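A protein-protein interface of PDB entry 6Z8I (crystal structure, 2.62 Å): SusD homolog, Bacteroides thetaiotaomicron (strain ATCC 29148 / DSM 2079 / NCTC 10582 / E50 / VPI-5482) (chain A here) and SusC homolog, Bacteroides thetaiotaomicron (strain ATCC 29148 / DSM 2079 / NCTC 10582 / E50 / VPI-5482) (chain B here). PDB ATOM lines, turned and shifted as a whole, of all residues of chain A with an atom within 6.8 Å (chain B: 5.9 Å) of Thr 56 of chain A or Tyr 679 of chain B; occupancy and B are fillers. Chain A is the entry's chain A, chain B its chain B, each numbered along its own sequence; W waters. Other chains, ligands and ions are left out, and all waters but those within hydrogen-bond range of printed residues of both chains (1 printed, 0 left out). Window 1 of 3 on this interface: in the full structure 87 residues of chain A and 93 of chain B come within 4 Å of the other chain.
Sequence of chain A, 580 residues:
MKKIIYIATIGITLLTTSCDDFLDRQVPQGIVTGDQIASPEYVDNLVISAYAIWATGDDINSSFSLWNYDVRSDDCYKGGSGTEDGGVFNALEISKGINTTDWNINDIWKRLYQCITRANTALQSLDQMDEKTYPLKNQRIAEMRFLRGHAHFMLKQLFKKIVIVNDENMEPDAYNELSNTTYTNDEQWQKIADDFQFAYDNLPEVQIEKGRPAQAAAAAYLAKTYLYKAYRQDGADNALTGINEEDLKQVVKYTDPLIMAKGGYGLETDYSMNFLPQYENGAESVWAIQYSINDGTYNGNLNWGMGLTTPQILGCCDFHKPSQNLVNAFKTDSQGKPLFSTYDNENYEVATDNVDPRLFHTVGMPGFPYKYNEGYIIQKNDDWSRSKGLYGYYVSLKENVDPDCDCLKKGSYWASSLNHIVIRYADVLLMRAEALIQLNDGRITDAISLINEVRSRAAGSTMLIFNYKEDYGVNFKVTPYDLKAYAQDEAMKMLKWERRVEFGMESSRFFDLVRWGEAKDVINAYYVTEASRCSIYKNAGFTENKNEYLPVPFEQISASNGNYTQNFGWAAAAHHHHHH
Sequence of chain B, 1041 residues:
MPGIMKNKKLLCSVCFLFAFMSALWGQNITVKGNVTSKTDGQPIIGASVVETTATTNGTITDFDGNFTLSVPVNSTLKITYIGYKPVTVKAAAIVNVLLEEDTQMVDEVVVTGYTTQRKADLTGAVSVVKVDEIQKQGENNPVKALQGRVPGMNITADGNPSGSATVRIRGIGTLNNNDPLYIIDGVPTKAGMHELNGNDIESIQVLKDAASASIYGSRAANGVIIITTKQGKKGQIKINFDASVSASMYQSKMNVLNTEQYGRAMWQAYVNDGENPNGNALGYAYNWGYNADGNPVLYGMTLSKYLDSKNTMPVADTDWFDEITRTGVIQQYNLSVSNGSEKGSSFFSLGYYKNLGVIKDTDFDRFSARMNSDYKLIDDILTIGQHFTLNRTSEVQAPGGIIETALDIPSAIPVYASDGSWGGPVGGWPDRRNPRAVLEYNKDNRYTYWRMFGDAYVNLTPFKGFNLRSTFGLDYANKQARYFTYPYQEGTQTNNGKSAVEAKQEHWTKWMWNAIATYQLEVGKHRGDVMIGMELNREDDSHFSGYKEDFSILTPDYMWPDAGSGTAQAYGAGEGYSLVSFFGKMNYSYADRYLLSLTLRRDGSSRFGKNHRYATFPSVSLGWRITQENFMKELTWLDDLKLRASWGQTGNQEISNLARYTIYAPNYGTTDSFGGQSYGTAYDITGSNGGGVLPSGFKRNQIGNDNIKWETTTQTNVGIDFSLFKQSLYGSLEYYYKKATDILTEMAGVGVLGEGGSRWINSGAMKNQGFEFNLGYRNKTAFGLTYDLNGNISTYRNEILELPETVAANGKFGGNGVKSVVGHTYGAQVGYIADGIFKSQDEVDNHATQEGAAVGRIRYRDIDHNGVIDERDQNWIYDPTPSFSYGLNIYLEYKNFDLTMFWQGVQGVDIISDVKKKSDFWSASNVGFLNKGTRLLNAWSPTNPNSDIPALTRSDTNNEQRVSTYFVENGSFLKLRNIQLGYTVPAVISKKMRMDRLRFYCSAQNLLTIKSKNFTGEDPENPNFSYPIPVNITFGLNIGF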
ATOM      1  N   SER A  49      20.455 -11.660  -6.366  1.00  0.00           N
ATOM      2  CA  SER A  49      19.069 -11.235  -6.295  1.00  0.00           C
ATOM      3  C   SER A  49      18.457 -11.567  -4.940  1.00  0.00           C
ATOM      4  O   SER A  49      17.778 -10.729  -4.332  1.00  0.00           O
ATOM      5  CB  SER A  49      18.289 -11.885  -7.426  1.00  0.00           C
ATOM      6  OG  SER A  49      17.114 -11.148  -7.652  1.00  0.00           O
ATOM      7  N   TYR A  51      20.101 -11.864  -2.068  1.00  0.00           N
ATOM      8  CA  TYR A  51      20.558 -10.868  -1.107  1.00  0.00           C
ATOM      9  C   TYR A  51      19.781  -9.576  -1.295  1.00  0.00           C
ATOM     10  O   TYR A  51      19.305  -8.976  -0.313  1.00  0.00           O
ATOM     11  CB  TYR A  51      22.047 -10.622  -1.251  1.00  0.00           C
ATOM     12  CG  TYR A  51      22.922 -11.696  -0.695  1.00  0.00           C
ATOM     13  CD1 TYR A  51      23.273 -11.712   0.664  1.00  0.00           C
ATOM     14  CD2 TYR A  51      23.461 -12.666  -1.519  1.00  0.00           C
ATOM     15  CE1 TYR A  51      24.102 -12.675   1.176  1.00  0.00           C
ATOM     16  CE2 TYR A  51      24.307 -13.649  -1.005  1.00  0.00           C
ATOM     17  CZ  TYR A  51      24.619 -13.640   0.339  1.00  0.00           C
ATOM     18  OH  TYR A  51      25.458 -14.600   0.836  1.00  0.00           O
ATOM     19  N   ALA A  52      19.593  -9.169  -2.569  1.00  0.00           N
ATOM     20  CA  ALA A  52      19.035  -7.857  -2.887  1.00  0.00           C
ATOM     21  C   ALA A  52      17.685  -7.630  -2.220  1.00  0.00           C
ATOM     22  O   ALA A  52      17.420  -6.540  -1.698  1.00  0.00           O
ATOM     23  CB  ALA A  52      18.911  -7.703  -4.397  1.00  0.00           C
ATOM     24  N   ILE A  53      16.815  -8.642  -2.207  1.00  0.00           N
ATOM     25  CA  ILE A  53      15.476  -8.408  -1.690  1.00  0.00           C
ATOM     26  C   ILE A  53      15.463  -8.058  -0.204  1.00  0.00           C
ATOM     27  O   ILE A  53      14.473  -7.502   0.274  1.00  0.00           O
ATOM     28  CB  ILE A  53      14.591  -9.619  -2.010  1.00  0.00           C
ATOM     29  CG1 ILE A  53      13.133  -9.316  -1.713  1.00  0.00           C
ATOM     30  CG2 ILE A  53      15.050 -10.859  -1.276  1.00  0.00           C
ATOM     31  CD1 ILE A  53      12.240 -10.365  -2.358  1.00  0.00           C
ATOM     32  N   TRP A  54      16.559  -8.313   0.535  1.00  0.00           N
ATOM     33  CA  TRP A  54      16.607  -7.899   1.935  1.00  0.00           C
ATOM     34  C   TRP A  54      16.722  -6.395   2.078  1.00  0.00           C
ATOM     35  O   TRP A  54      16.317  -5.849   3.107  1.00  0.00           O
ATOM     36  CB  TRP A  54      17.747  -8.631   2.654  1.00  0.00           C
ATOM     37  CG  TRP A  54      17.325 -10.043   2.847  1.00  0.00           C
ATOM     38  CD1 TRP A  54      17.711 -11.140   2.121  1.00  0.00           C
ATOM     39  CD2 TRP A  54      16.324 -10.498   3.756  1.00  0.00           C
ATOM     40  NE1 TRP A  54      17.045 -12.257   2.565  1.00  0.00           N
ATOM     41  CE2 TRP A  54      16.181 -11.886   3.564  1.00  0.00           C
ATOM     42  CE3 TRP A  54      15.543  -9.865   4.729  1.00  0.00           C
ATOM     43  CZ2 TRP A  54      15.286 -12.653   4.314  1.00  0.00           C
ATOM     44  CZ3 TRP A  54      14.656 -10.619   5.462  1.00  0.00           C
ATOM     45  CH2 TRP A  54      14.537 -12.004   5.261  1.00  0.00           C
ATOM     46  N   ALA A  55      17.212  -5.716   1.046  1.00  0.00           N
ATOM     47  CA  ALA A  55      17.232  -4.258   0.966  1.00  0.00           C
ATOM     48  C   ALA A  55      15.996  -3.707   0.251  1.00  0.00           C
ATOM     49  O   ALA A  55      15.415  -2.701   0.675  1.00  0.00           O
ATOM     50  CB  ALA A  55      18.522  -3.799   0.253  1.00  0.00           C
ATOM     51  N   THR A  56      15.550  -4.375  -0.802  1.00  0.00           N
ATOM     52  CA  THR A  56      14.544  -3.819  -1.699  1.00  0.00           C
ATOM     53  C   THR A  56      13.118  -4.362  -1.518  1.00  0.00           C
ATOM     54  O   THR A  56      12.217  -3.917  -2.226  1.00  0.00           O
ATOM     55  CB  THR A  56      15.013  -4.050  -3.134  1.00  0.00           C
ATOM     56  OG1 THR A  56      14.905  -5.446  -3.475  1.00  0.00           O
ATOM     57  CG2 THR A  56      16.475  -3.631  -3.236  1.00  0.00           C
ATOM     58  N   GLY A  57      12.874  -5.280  -0.585  1.00  0.00           N
ATOM     59  CA  GLY A  57      11.623  -6.025  -0.530  1.00  0.00           C
ATOM     60  C   GLY A  57      10.661  -5.567   0.553  1.00  0.00           C
ATOM     61  O   GLY A  57       9.524  -6.062   0.652  1.00  0.00           O
ATOM     62  N   ASP A  58      11.095  -4.601   1.360  1.00  0.00           N
ATOM     63  CA  ASP A  58      10.287  -4.026   2.426  1.00  0.00           C
ATOM     64  C   ASP A  58       9.883  -2.608   2.059  1.00  0.00           C
ATOM     65  O   ASP A  58      10.329  -2.059   1.054  1.00  0.00           O
ATOM     66  CB  ASP A  58      11.037  -4.025   3.775  1.00  0.00           C
ATOM     67  CG  ASP A  58      12.456  -3.474   3.686  1.00  0.00           C
ATOM     68  OD1 ASP A  58      12.901  -3.113   2.582  1.00  0.00           O
ATOM     69  OD2 ASP A  58      13.130  -3.390   4.739  1.00  0.00           O
ATOM     70  N   ASP A  59       9.026  -2.020   2.892  1.00  0.00           N
ATOM     71  CA  ASP A  59       8.642  -0.614   2.782  1.00  0.00           C
ATOM     72  C   ASP A  59       8.463  -0.023   4.182  1.00  0.00           C
ATOM     73  O   ASP A  59       8.680  -0.687   5.198  1.00  0.00           O
ATOM     74  CB  ASP A  59       7.368  -0.453   1.925  1.00  0.00           C
ATOM     75  CG  ASP A  59       6.073  -0.804   2.680  1.00  0.00           C
ATOM     76  OD1 ASP A  59       6.148  -1.402   3.783  1.00  0.00           O
ATOM     77  OD2 ASP A  59       4.964  -0.492   2.157  1.00  0.00           O
ATOM     78  N   PHE A  64      12.109  -4.892   7.556  1.00  0.00           N
ATOM     79  CA  PHE A  64      12.741  -6.157   7.901  1.00  0.00           C
ATOM     80  C   PHE A  64      13.544  -6.084   9.189  1.00  0.00           C
ATOM     81  O   PHE A  64      14.065  -7.113   9.640  1.00  0.00           O
ATOM     82  CB  PHE A  64      13.620  -6.611   6.746  1.00  0.00           C
ATOM     83  CG  PHE A  64      12.834  -7.069   5.544  1.00  0.00           C
ATOM     84  CD1 PHE A  64      11.494  -7.413   5.671  1.00  0.00           C
ATOM     85  CD2 PHE A  64      13.435  -7.176   4.292  1.00  0.00           C
ATOM     86  CE1 PHE A  64      10.773  -7.857   4.575  1.00  0.00           C
ATOM     87  CE2 PHE A  64      12.709  -7.619   3.192  1.00  0.00           C
ATOM     88  CZ  PHE A  64      11.383  -7.964   3.340  1.00  0.00           C
ATOM     89  N   ARG A 111       5.716 -10.537   2.500  1.00  0.00           N
ATOM     90  CA  ARG A 111       6.999  -9.987   2.092  1.00  0.00           C
ATOM     91  C   ARG A 111       8.151 -10.913   2.449  1.00  0.00           C
ATOM     92  O   ARG A 111       9.098 -11.053   1.665  1.00  0.00           O
ATOM     93  CB  ARG A 111       7.186  -8.615   2.725  1.00  0.00           C
ATOM     94  CG  ARG A 111       6.481  -7.513   1.962  1.00  0.00           C
ATOM     95  CD  ARG A 111       6.855  -6.171   2.550  1.00  0.00           C
ATOM     96  NE  ARG A 111       5.791  -5.199   2.356  1.00  0.00           N
ATOM     97  CZ  ARG A 111       5.760  -4.382   1.320  1.00  0.00           C
ATOM     98  NH1 ARG A 111       6.739  -4.446   0.422  1.00  0.00           N
ATOM     99  NH2 ARG A 111       4.773  -3.514   1.192  1.00  0.00           N
ATOM    100  N   GLN A 114       8.407 -13.707   0.064  1.00  0.00           N
ATOM    101  CA  GLN A 114       9.051 -13.324  -1.193  1.00  0.00           C
ATOM    102  C   GLN A 114      10.576 -13.451  -1.086  1.00  0.00           C
ATOM    103  O   GLN A 114      11.236 -13.932  -2.026  1.00  0.00           O
ATOM    104  CB  GLN A 114       8.618 -11.906  -1.596  1.00  0.00           C
ATOM    105  CG  GLN A 114       7.200 -11.860  -2.186  1.00  0.00           C
ATOM    106  CD  GLN A 114       6.636 -10.462  -2.475  1.00  0.00           C
ATOM    107  OE1 GLN A 114       7.211  -9.446  -2.093  1.00  0.00           O
ATOM    108  NE2 GLN A 114       5.491 -10.419  -3.161  1.00  0.00           N
ATOM    109  N   ARG A 118      13.355 -15.944  -3.793  1.00  0.00           N
ATOM    110  CA  ARG A 118      14.643 -15.758  -4.457  1.00  0.00           C
ATOM    111  C   ARG A 118      15.690 -16.733  -3.918  1.00  0.00           C
ATOM    112  O   ARG A 118      16.467 -17.306  -4.693  1.00  0.00           O
ATOM    113  CB  ARG A 118      15.109 -14.308  -4.322  1.00  0.00           C
ATOM    114  CG  ARG A 118      14.090 -13.265  -4.786  1.00  0.00           C
ATOM    115  CD  ARG A 118      14.779 -12.076  -5.440  1.00  0.00           C
ATOM    116  NE  ARG A 118      13.862 -10.964  -5.667  1.00  0.00           N
ATOM    117  CZ  ARG A 118      14.225  -9.686  -5.753  1.00  0.00           C
ATOM    118  NH1 ARG A 118      15.507  -9.335  -5.625  1.00  0.00           N
ATOM    119  NH2 ARG A 118      13.294  -8.757  -5.969  1.00  0.00           N
ATOM    120  N   TYR A 291      22.895  -1.816   3.029  1.00  0.00           N
ATOM    121  CA  TYR A 291      22.319  -0.621   2.431  1.00  0.00           C
ATOM    122  C   TYR A 291      23.413   0.245   1.820  1.00  0.00           C
ATOM    123  O   TYR A 291      24.491   0.400   2.396  1.00  0.00           O
ATOM    124  CB  TYR A 291      21.528   0.146   3.499  1.00  0.00           C
ATOM    125  CG  TYR A 291      20.318  -0.639   3.990  1.00  0.00           C
ATOM    126  CD1 TYR A 291      20.284  -1.193   5.270  1.00  0.00           C
ATOM    127  CD2 TYR A 291      19.212  -0.846   3.155  1.00  0.00           C
ATOM    128  CE1 TYR A 291      19.168  -1.926   5.714  1.00  0.00           C
ATOM    129  CE2 TYR A 291      18.110  -1.555   3.593  1.00  0.00           C
ATOM    130  CZ  TYR A 291      18.087  -2.105   4.872  1.00  0.00           C
ATOM    131  OH  TYR A 291      16.971  -2.840   5.281  1.00  0.00           O
ATOM    132  N   THR A 297      20.910   2.753  -8.474  1.00  0.00           N
ATOM    133  CA  THR A 297      19.477   2.669  -8.269  1.00  0.00           C
ATOM    134  C   THR A 297      18.873   4.072  -8.254  1.00  0.00           C
ATOM    135  O   THR A 297      19.567   5.077  -8.163  1.00  0.00           O
ATOM    136  CB  THR A 297      19.145   1.922  -6.972  1.00  0.00           C
ATOM    137  OG1 THR A 297      19.352   2.793  -5.852  1.00  0.00           O
ATOM    138  CG2 THR A 297      20.010   0.674  -6.805  1.00  0.00           C
ATOM    139  N   ASN A 301      20.125   2.178  -2.672  1.00  0.00           N
ATOM    140  CA  ASN A 301      19.569   1.104  -1.853  1.00  0.00           C
ATOM    141  C   ASN A 301      19.650   1.540  -0.392  1.00  0.00           C
ATOM    142  O   ASN A 301      20.394   0.993   0.427  1.00  0.00           O
ATOM    143  CB  ASN A 301      20.299  -0.211  -2.077  1.00  0.00           C
ATOM    144  CG  ASN A 301      19.743  -1.009  -3.224  1.00  0.00           C
ATOM    145  OD1 ASN A 301      18.675  -0.695  -3.785  1.00  0.00           O
ATOM    146  ND2 ASN A 301      20.460  -2.068  -3.583  1.00  0.00           N
ATOM    147  N   LEU A 302      18.871   2.564  -0.072  1.00  0.00           N
ATOM    148  CA  LEU A 302      18.843   3.010   1.307  1.00  0.00           C
ATOM    149  C   LEU A 302      17.851   2.170   2.106  1.00  0.00           C
ATOM    150  O   LEU A 302      17.074   1.364   1.571  1.00  0.00           O
ATOM    151  CB  LEU A 302      18.503   4.502   1.403  1.00  0.00           C
ATOM    152  CG  LEU A 302      19.290   5.405   0.423  1.00  0.00           C
ATOM    153  CD1 LEU A 302      18.808   6.841   0.522  1.00  0.00           C
ATOM    154  CD2 LEU A 302      20.847   5.331   0.581  1.00  0.00           C
ATOM    155  N   TRP A 304      14.980   2.311   3.283  1.00  0.00           N
ATOM    156  CA  TRP A 304      13.677   2.963   3.202  1.00  0.00           C
ATOM    157  C   TRP A 304      12.722   2.468   4.283  1.00  0.00           C
ATOM    158  O   TRP A 304      11.770   3.178   4.638  1.00  0.00           O
ATOM    159  CB  TRP A 304      13.077   2.730   1.817  1.00  0.00           C
ATOM    160  CG  TRP A 304      13.984   3.140   0.725  1.00  0.00           C
ATOM    161  CD1 TRP A 304      14.676   2.327  -0.126  1.00  0.00           C
ATOM    162  CD2 TRP A 304      14.309   4.488   0.347  1.00  0.00           C
ATOM    163  NE1 TRP A 304      15.426   3.089  -1.003  1.00  0.00           N
ATOM    164  CE2 TRP A 304      15.220   4.416  -0.725  1.00  0.00           C
ATOM    165  CE3 TRP A 304      13.940   5.745   0.834  1.00  0.00           C
ATOM    166  CZ2 TRP A 304      15.749   5.550  -1.328  1.00  0.00           C
ATOM    167  CZ3 TRP A 304      14.471   6.861   0.238  1.00  0.00           C
ATOM    168  CH2 TRP A 304      15.363   6.757  -0.840  1.00  0.00           C
ATOM    169  N   ASN B 667      15.343  -5.919 -13.486  1.00  0.00           N
ATOM    170  CA  ASN B 667      14.942  -4.953 -12.460  1.00  0.00           C
ATOM    171  C   ASN B 667      16.030  -4.615 -11.423  1.00  0.00           C
ATOM    172  O   ASN B 667      15.904  -4.952 -10.232  1.00  0.00           O
ATOM    173  CB  ASN B 667      13.684  -5.445 -11.732  1.00  0.00           C
ATOM    174  CG  ASN B 667      12.994  -4.317 -11.002  1.00  0.00           C
ATOM    175  OD1 ASN B 667      12.785  -3.249 -11.580  1.00  0.00           O
ATOM    176  ND2 ASN B 667      12.739  -4.492  -9.714  1.00  0.00           N
ATOM    177  N   TYR B 668      17.095  -3.944 -11.889  1.00  0.00           N
ATOM    178  CA  TYR B 668      18.184  -3.499 -11.023  1.00  0.00           C
ATOM    179  C   TYR B 668      17.675  -2.581  -9.921  1.00  0.00           C
ATOM    180  O   TYR B 668      18.122  -2.678  -8.766  1.00  0.00           O
ATOM    181  CB  TYR B 668      19.241  -2.805 -11.877  1.00  0.00           C
ATOM    182  CG  TYR B 668      20.496  -2.247 -11.207  1.00  0.00           C
ATOM    183  CD1 TYR B 668      20.470  -1.028 -10.511  1.00  0.00           C
ATOM    184  CD2 TYR B 668      21.727  -2.884 -11.361  1.00  0.00           C
ATOM    185  CE1 TYR B 668      21.625  -0.487  -9.948  1.00  0.00           C
ATOM    186  CE2 TYR B 668      22.890  -2.352 -10.804  1.00  0.00           C
ATOM    187  CZ  TYR B 668      22.838  -1.151 -10.101  1.00  0.00           C
ATOM    188  OH  TYR B 668      24.004  -0.634  -9.549  1.00  0.00           O
ATOM    189  N   GLY B 669      16.743  -1.686 -10.258  1.00  0.00           N
ATOM    190  CA  GLY B 669      16.097  -0.843  -9.266  1.00  0.00           C
ATOM    191  C   GLY B 669      16.167   0.629  -9.617  1.00  0.00           C
ATOM    192  O   GLY B 669      16.396   1.506  -8.771  1.00  0.00           O
ATOM    193  N   GLY B 676       9.906   2.514  -0.454  1.00  0.00           N
ATOM    194  CA  GLY B 676      10.583   1.238  -0.568  1.00  0.00           C
ATOM    195  C   GLY B 676      10.090   0.481  -1.791  1.00  0.00           C
ATOM    196  O   GLY B 676       9.799   1.088  -2.830  1.00  0.00           O
ATOM    197  N   GLN B 677       9.978  -0.842  -1.657  1.00  0.00           N
ATOM    198  CA  GLN B 677       9.335  -1.704  -2.653  1.00  0.00           C
ATOM    199  C   GLN B 677       9.963  -1.621  -4.027  1.00  0.00           C
ATOM    200  O   GLN B 677       9.290  -1.847  -5.028  1.00  0.00           O
ATOM    201  CB  GLN B 677       7.841  -1.393  -2.795  1.00  0.00           C
ATOM    202  CG  GLN B 677       7.109  -1.480  -1.505  1.00  0.00           C
ATOM    203  CD  GLN B 677       5.624  -1.315  -1.679  1.00  0.00           C
ATOM    204  OE1 GLN B 677       4.848  -2.256  -1.450  1.00  0.00           O
ATOM    205  NE2 GLN B 677       5.209  -0.112  -2.073  1.00  0.00           N
ATOM    206  N   SER B 678      11.229  -1.256  -4.136  1.00  0.00           N
ATOM    207  CA  SER B 678      11.887  -1.338  -5.434  1.00  0.00           C
ATOM    208  C   SER B 678      11.836  -2.757  -5.987  1.00  0.00           C
ATOM    209  O   SER B 678      11.609  -2.961  -7.182  1.00  0.00           O
ATOM    210  CB  SER B 678      13.317  -0.863  -5.300  1.00  0.00           C
ATOM    211  OG  SER B 678      14.159  -1.566  -6.192  1.00  0.00           O
ATOM    212  N   TYR B 679      12.009  -3.749  -5.128  1.00  0.00           N
ATOM    213  CA  TYR B 679      12.263  -5.113  -5.560  1.00  0.00           C
ATOM    214  C   TYR B 679      13.424  -5.180  -6.538  1.00  0.00           C
ATOM    215  O   TYR B 679      13.451  -6.031  -7.429  1.00  0.00           O
ATOM    216  CB  TYR B 679      11.002  -5.754  -6.144  1.00  0.00           C
ATOM    217  CG  TYR B 679       9.886  -5.809  -5.125  1.00  0.00           C
ATOM    218  CD1 TYR B 679       9.960  -6.660  -4.037  1.00  0.00           C
ATOM    219  CD2 TYR B 679       8.799  -4.962  -5.218  1.00  0.00           C
ATOM    220  CE1 TYR B 679       8.957  -6.692  -3.090  1.00  0.00           C
ATOM    221  CE2 TYR B 679       7.801  -4.978  -4.280  1.00  0.00           C
ATOM    222  CZ  TYR B 679       7.872  -5.848  -3.218  1.00  0.00           C
ATOM    223  OH  TYR B 679       6.847  -5.866  -2.292  1.00  0.00           O
ATOM    224  N   GLY B 680      14.406  -4.292  -6.360  1.00  0.00           N
ATOM    225  CA  GLY B 680      15.606  -4.355  -7.172  1.00  0.00           C
ATOM    226  C   GLY B 680      16.416  -5.609  -6.901  1.00  0.00           C
ATOM    227  O   GLY B 680      16.338  -6.223  -5.823  1.00  0.00           O
ATOM    228  N   THR B 681      17.190  -6.008  -7.915  1.00  0.00           N
ATOM    229  CA  THR B 681      18.083  -7.151  -7.811  1.00  0.00           C
ATOM    230  C   THR B 681      19.536  -6.744  -7.598  1.00  0.00           C
ATOM    231  O   THR B 681      20.411  -7.610  -7.597  1.00  0.00           O
ATOM    232  CB  THR B 681      17.978  -8.048  -9.059  1.00  0.00           C
ATOM    233  OG1 THR B 681      18.580  -7.401 -10.186  1.00  0.00           O
ATOM    234  CG2 THR B 681      16.557  -8.366  -9.380  1.00  0.00           C
ATOM    235  N   ALA B 682      19.813  -5.456  -7.429  1.00  0.00           N
ATOM    236  CA  ALA B 682      21.163  -4.988  -7.155  1.00  0.00           C
ATOM    237  C   ALA B 682      21.427  -4.986  -5.655  1.00  0.00           C
ATOM    238  O   ALA B 682      20.586  -4.546  -4.867  1.00  0.00           O
ATOM    239  CB  ALA B 682      21.365  -3.582  -7.703  1.00  0.00           C
ATOM    240  N   LYS B 699      14.572 -11.131 -11.127  1.00  0.00           N
ATOM    241  CA  LYS B 699      13.437 -11.420 -10.261  1.00  0.00           C
ATOM    242  C   LYS B 699      12.231 -11.835 -11.114  1.00  0.00           C
ATOM    243  O   LYS B 699      12.119 -11.459 -12.291  1.00  0.00           O
ATOM    244  CB  LYS B 699      13.087 -10.211  -9.391  1.00  0.00           C
ATOM    245  CG  LYS B 699      12.077  -9.286 -10.095  1.00  0.00           C
ATOM    246  CD  LYS B 699      11.495  -8.261  -9.155  1.00  0.00           C
ATOM    247  CE  LYS B 699      10.067  -7.962  -9.519  1.00  0.00           C
ATOM    248  NZ  LYS B 699       9.833  -6.858 -10.469  1.00  0.00           N
ATOM    249  N   GLU B 755       7.313 -14.101  -4.591  1.00  0.00           N
ATOM    250  CA  GLU B 755       7.454 -13.067  -5.613  1.00  0.00           C
ATOM    251  C   GLU B 755       7.116 -13.622  -6.992  1.00  0.00           C
ATOM    252  O   GLU B 755       7.559 -14.713  -7.373  1.00  0.00           O
ATOM    253  CB  GLU B 755       8.876 -12.507  -5.600  1.00  0.00           C
ATOM    254  CG  GLU B 755       9.201 -11.589  -6.755  1.00  0.00           C
ATOM    255  CD  GLU B 755      10.555 -10.919  -6.612  1.00  0.00           C
ATOM    256  OE1 GLU B 755      11.577 -11.641  -6.683  1.00  0.00           O
ATOM    257  OE2 GLU B 755      10.592  -9.676  -6.444  1.00  0.00           O
HETATM  258  O   HOH W   1      16.682  -0.635  -5.394  1.00  0.00           O
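The backbone carbonyl oxygen of Thr 56 of chain A sits at hydrogen-bond distance from the backbone NH of Tyr 679 of chain B.
The side-chain hydroxyl of Thr 56 of chain A sits at hydrogen-bond distance from the backbone carbonyl oxygen of Gly 680 of chain B (2.9 Å).
N of Gln 677 of chain B sits at hydrogen-bond distance from O of Asp 58 of chain A, at 3.0 Å.
The guanidinium group (NH2) of Arg 111 of chain A sits at hydrogen-bond distance from the side-chain amide oxygen (OE1) of Gln 677 of chain B (2.9 Å).
The side-chain hydroxyl (OH) of Tyr 679 of chain B sits at hydrogen-bond distance from the guanidinium group (NH1) of Arg 111 of chain A (3.1 Å).
The backbone carbonyl oxygen (O) of Tyr 679 of chain B sits at hydrogen-bond distance from the guanidinium group (NH2) of Arg 118 of chain A, at 3.1 Å.
The side-chain amide nitrogen of Asn 301 of chain A is in hydrogen-bond range of the backbone carbonyl oxygen of Ala 682 of chain B (2.8 Å).
The backbone carbonyl oxygen (O) of Gly 680 of chain B lies within hydrogen-bond range of the guanidinium group (NH1) of Arg 118 of chain A (3.2 Å).
The guanidinium group (NE) of Arg 118 of chain A is in salt-bridge range of the side-chain carboxylate (OE1) of Glu 755 of chain B (2.6 Å).
The backbone carbonyl oxygen (O) of Thr 56 of chain A sits at hydrogen-bond distance from the backbone NH (N) of Ser 678 of chain B (3.4 Å).
OD2 of Asp 59 of chain A lies within salt-bridge range of NH2 of Arg 111 of chain A, 3.2 Å away.
The backbone carbonyl oxygen (O) of Asn 667 of chain B lies within hydrogen-bond range of the backbone NH (N) of Thr 681 of chain B (2.9 Å).
OG of Ser 678 of chain B sits at hydrogen-bond distance from N of Gly 680 of chain B (2.7 Å).
The side-chain carboxylate (OD2) of Asp 58 of chain A is in hydrogen-bond range of the backbone NH (N) of Phe 64 of chain A (3.4 Å).
Among the printed residues, merely in contact across the chains: Gln 114 of chain A with Glu 755 of chain B (3.3 Å), Ala 52 of chain A with Gly 680 of chain B (3.3 Å), Thr 297 of chain A with Gly 669 of chain B (3.3 Å), Ser 49 of chain A with Thr 681 of chain B (3.3 Å), Ala 52 of chain A with Thr 681 of chain B (3.4 Å), Gln 114 of chain A with Tyr 679 of chain B (3.4 Å), Asp 59 of chain A with Gln 677 of chain B (3.6 Å), Ala 52 of chain A with Ala 682 of chain B (3.6 Å), Thr 297 of chain A with Tyr 668 of chain B (3.6 Å), Thr 56 of chain A with Gln 677 of chain B (3.7 Å), Asp 58 of chain A with Gly 676 of chain B (3.7 Å), Arg 118 of chain A with Lys 699 of chain B (3.7 Å), Gly 57 of chain A with Tyr 679 of chain B (3.8 Å) and Trp 304 of chain A with Gly 676 of chain B (3.8 Å).
Of chain B, only Gln 677, Ser 678, Tyr 679 and Gly 680 come within 4 Å of Thr 56 of chain A.
Printed residues of chain B within 4 Å of Arg 111 of chain A: Gln 677 (2.9 Å) and Tyr 679 (3.1 Å).
Printed residues of chain B within 4 Å of Arg 118 of chain A: Tyr 679 (3.1 Å), Gly 680 (3.2 Å), Lys 699 (3.7 Å) and Glu 755 (2.6 Å).
The nearest residue of chain B that does not touch Thr 56 of chain A is Ala 682 of chain B (4.5 Å).
Of the 19 printed residues of chain A, 12 touch a printed residue of chain B.
Hydrophobic or aromatic side chains of chain A within 4 Å of the printed part of chain B: Ala 52 and Trp 304.
Of the 12 printed residues of chain B, 11 touch a printed residue of chain A.
Among the printed residues, Asp or Glu carboxylates within 4 Å of a Lys or Arg side-chain nitrogen of the other chain: Arg 118 of chain A with Glu 755 of chain B (2.6 Å).
Water W1 bridges OD1 of Asn 301 of chain A (2.6 Å) and OG of Ser 678 of chain B (2.8 Å).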
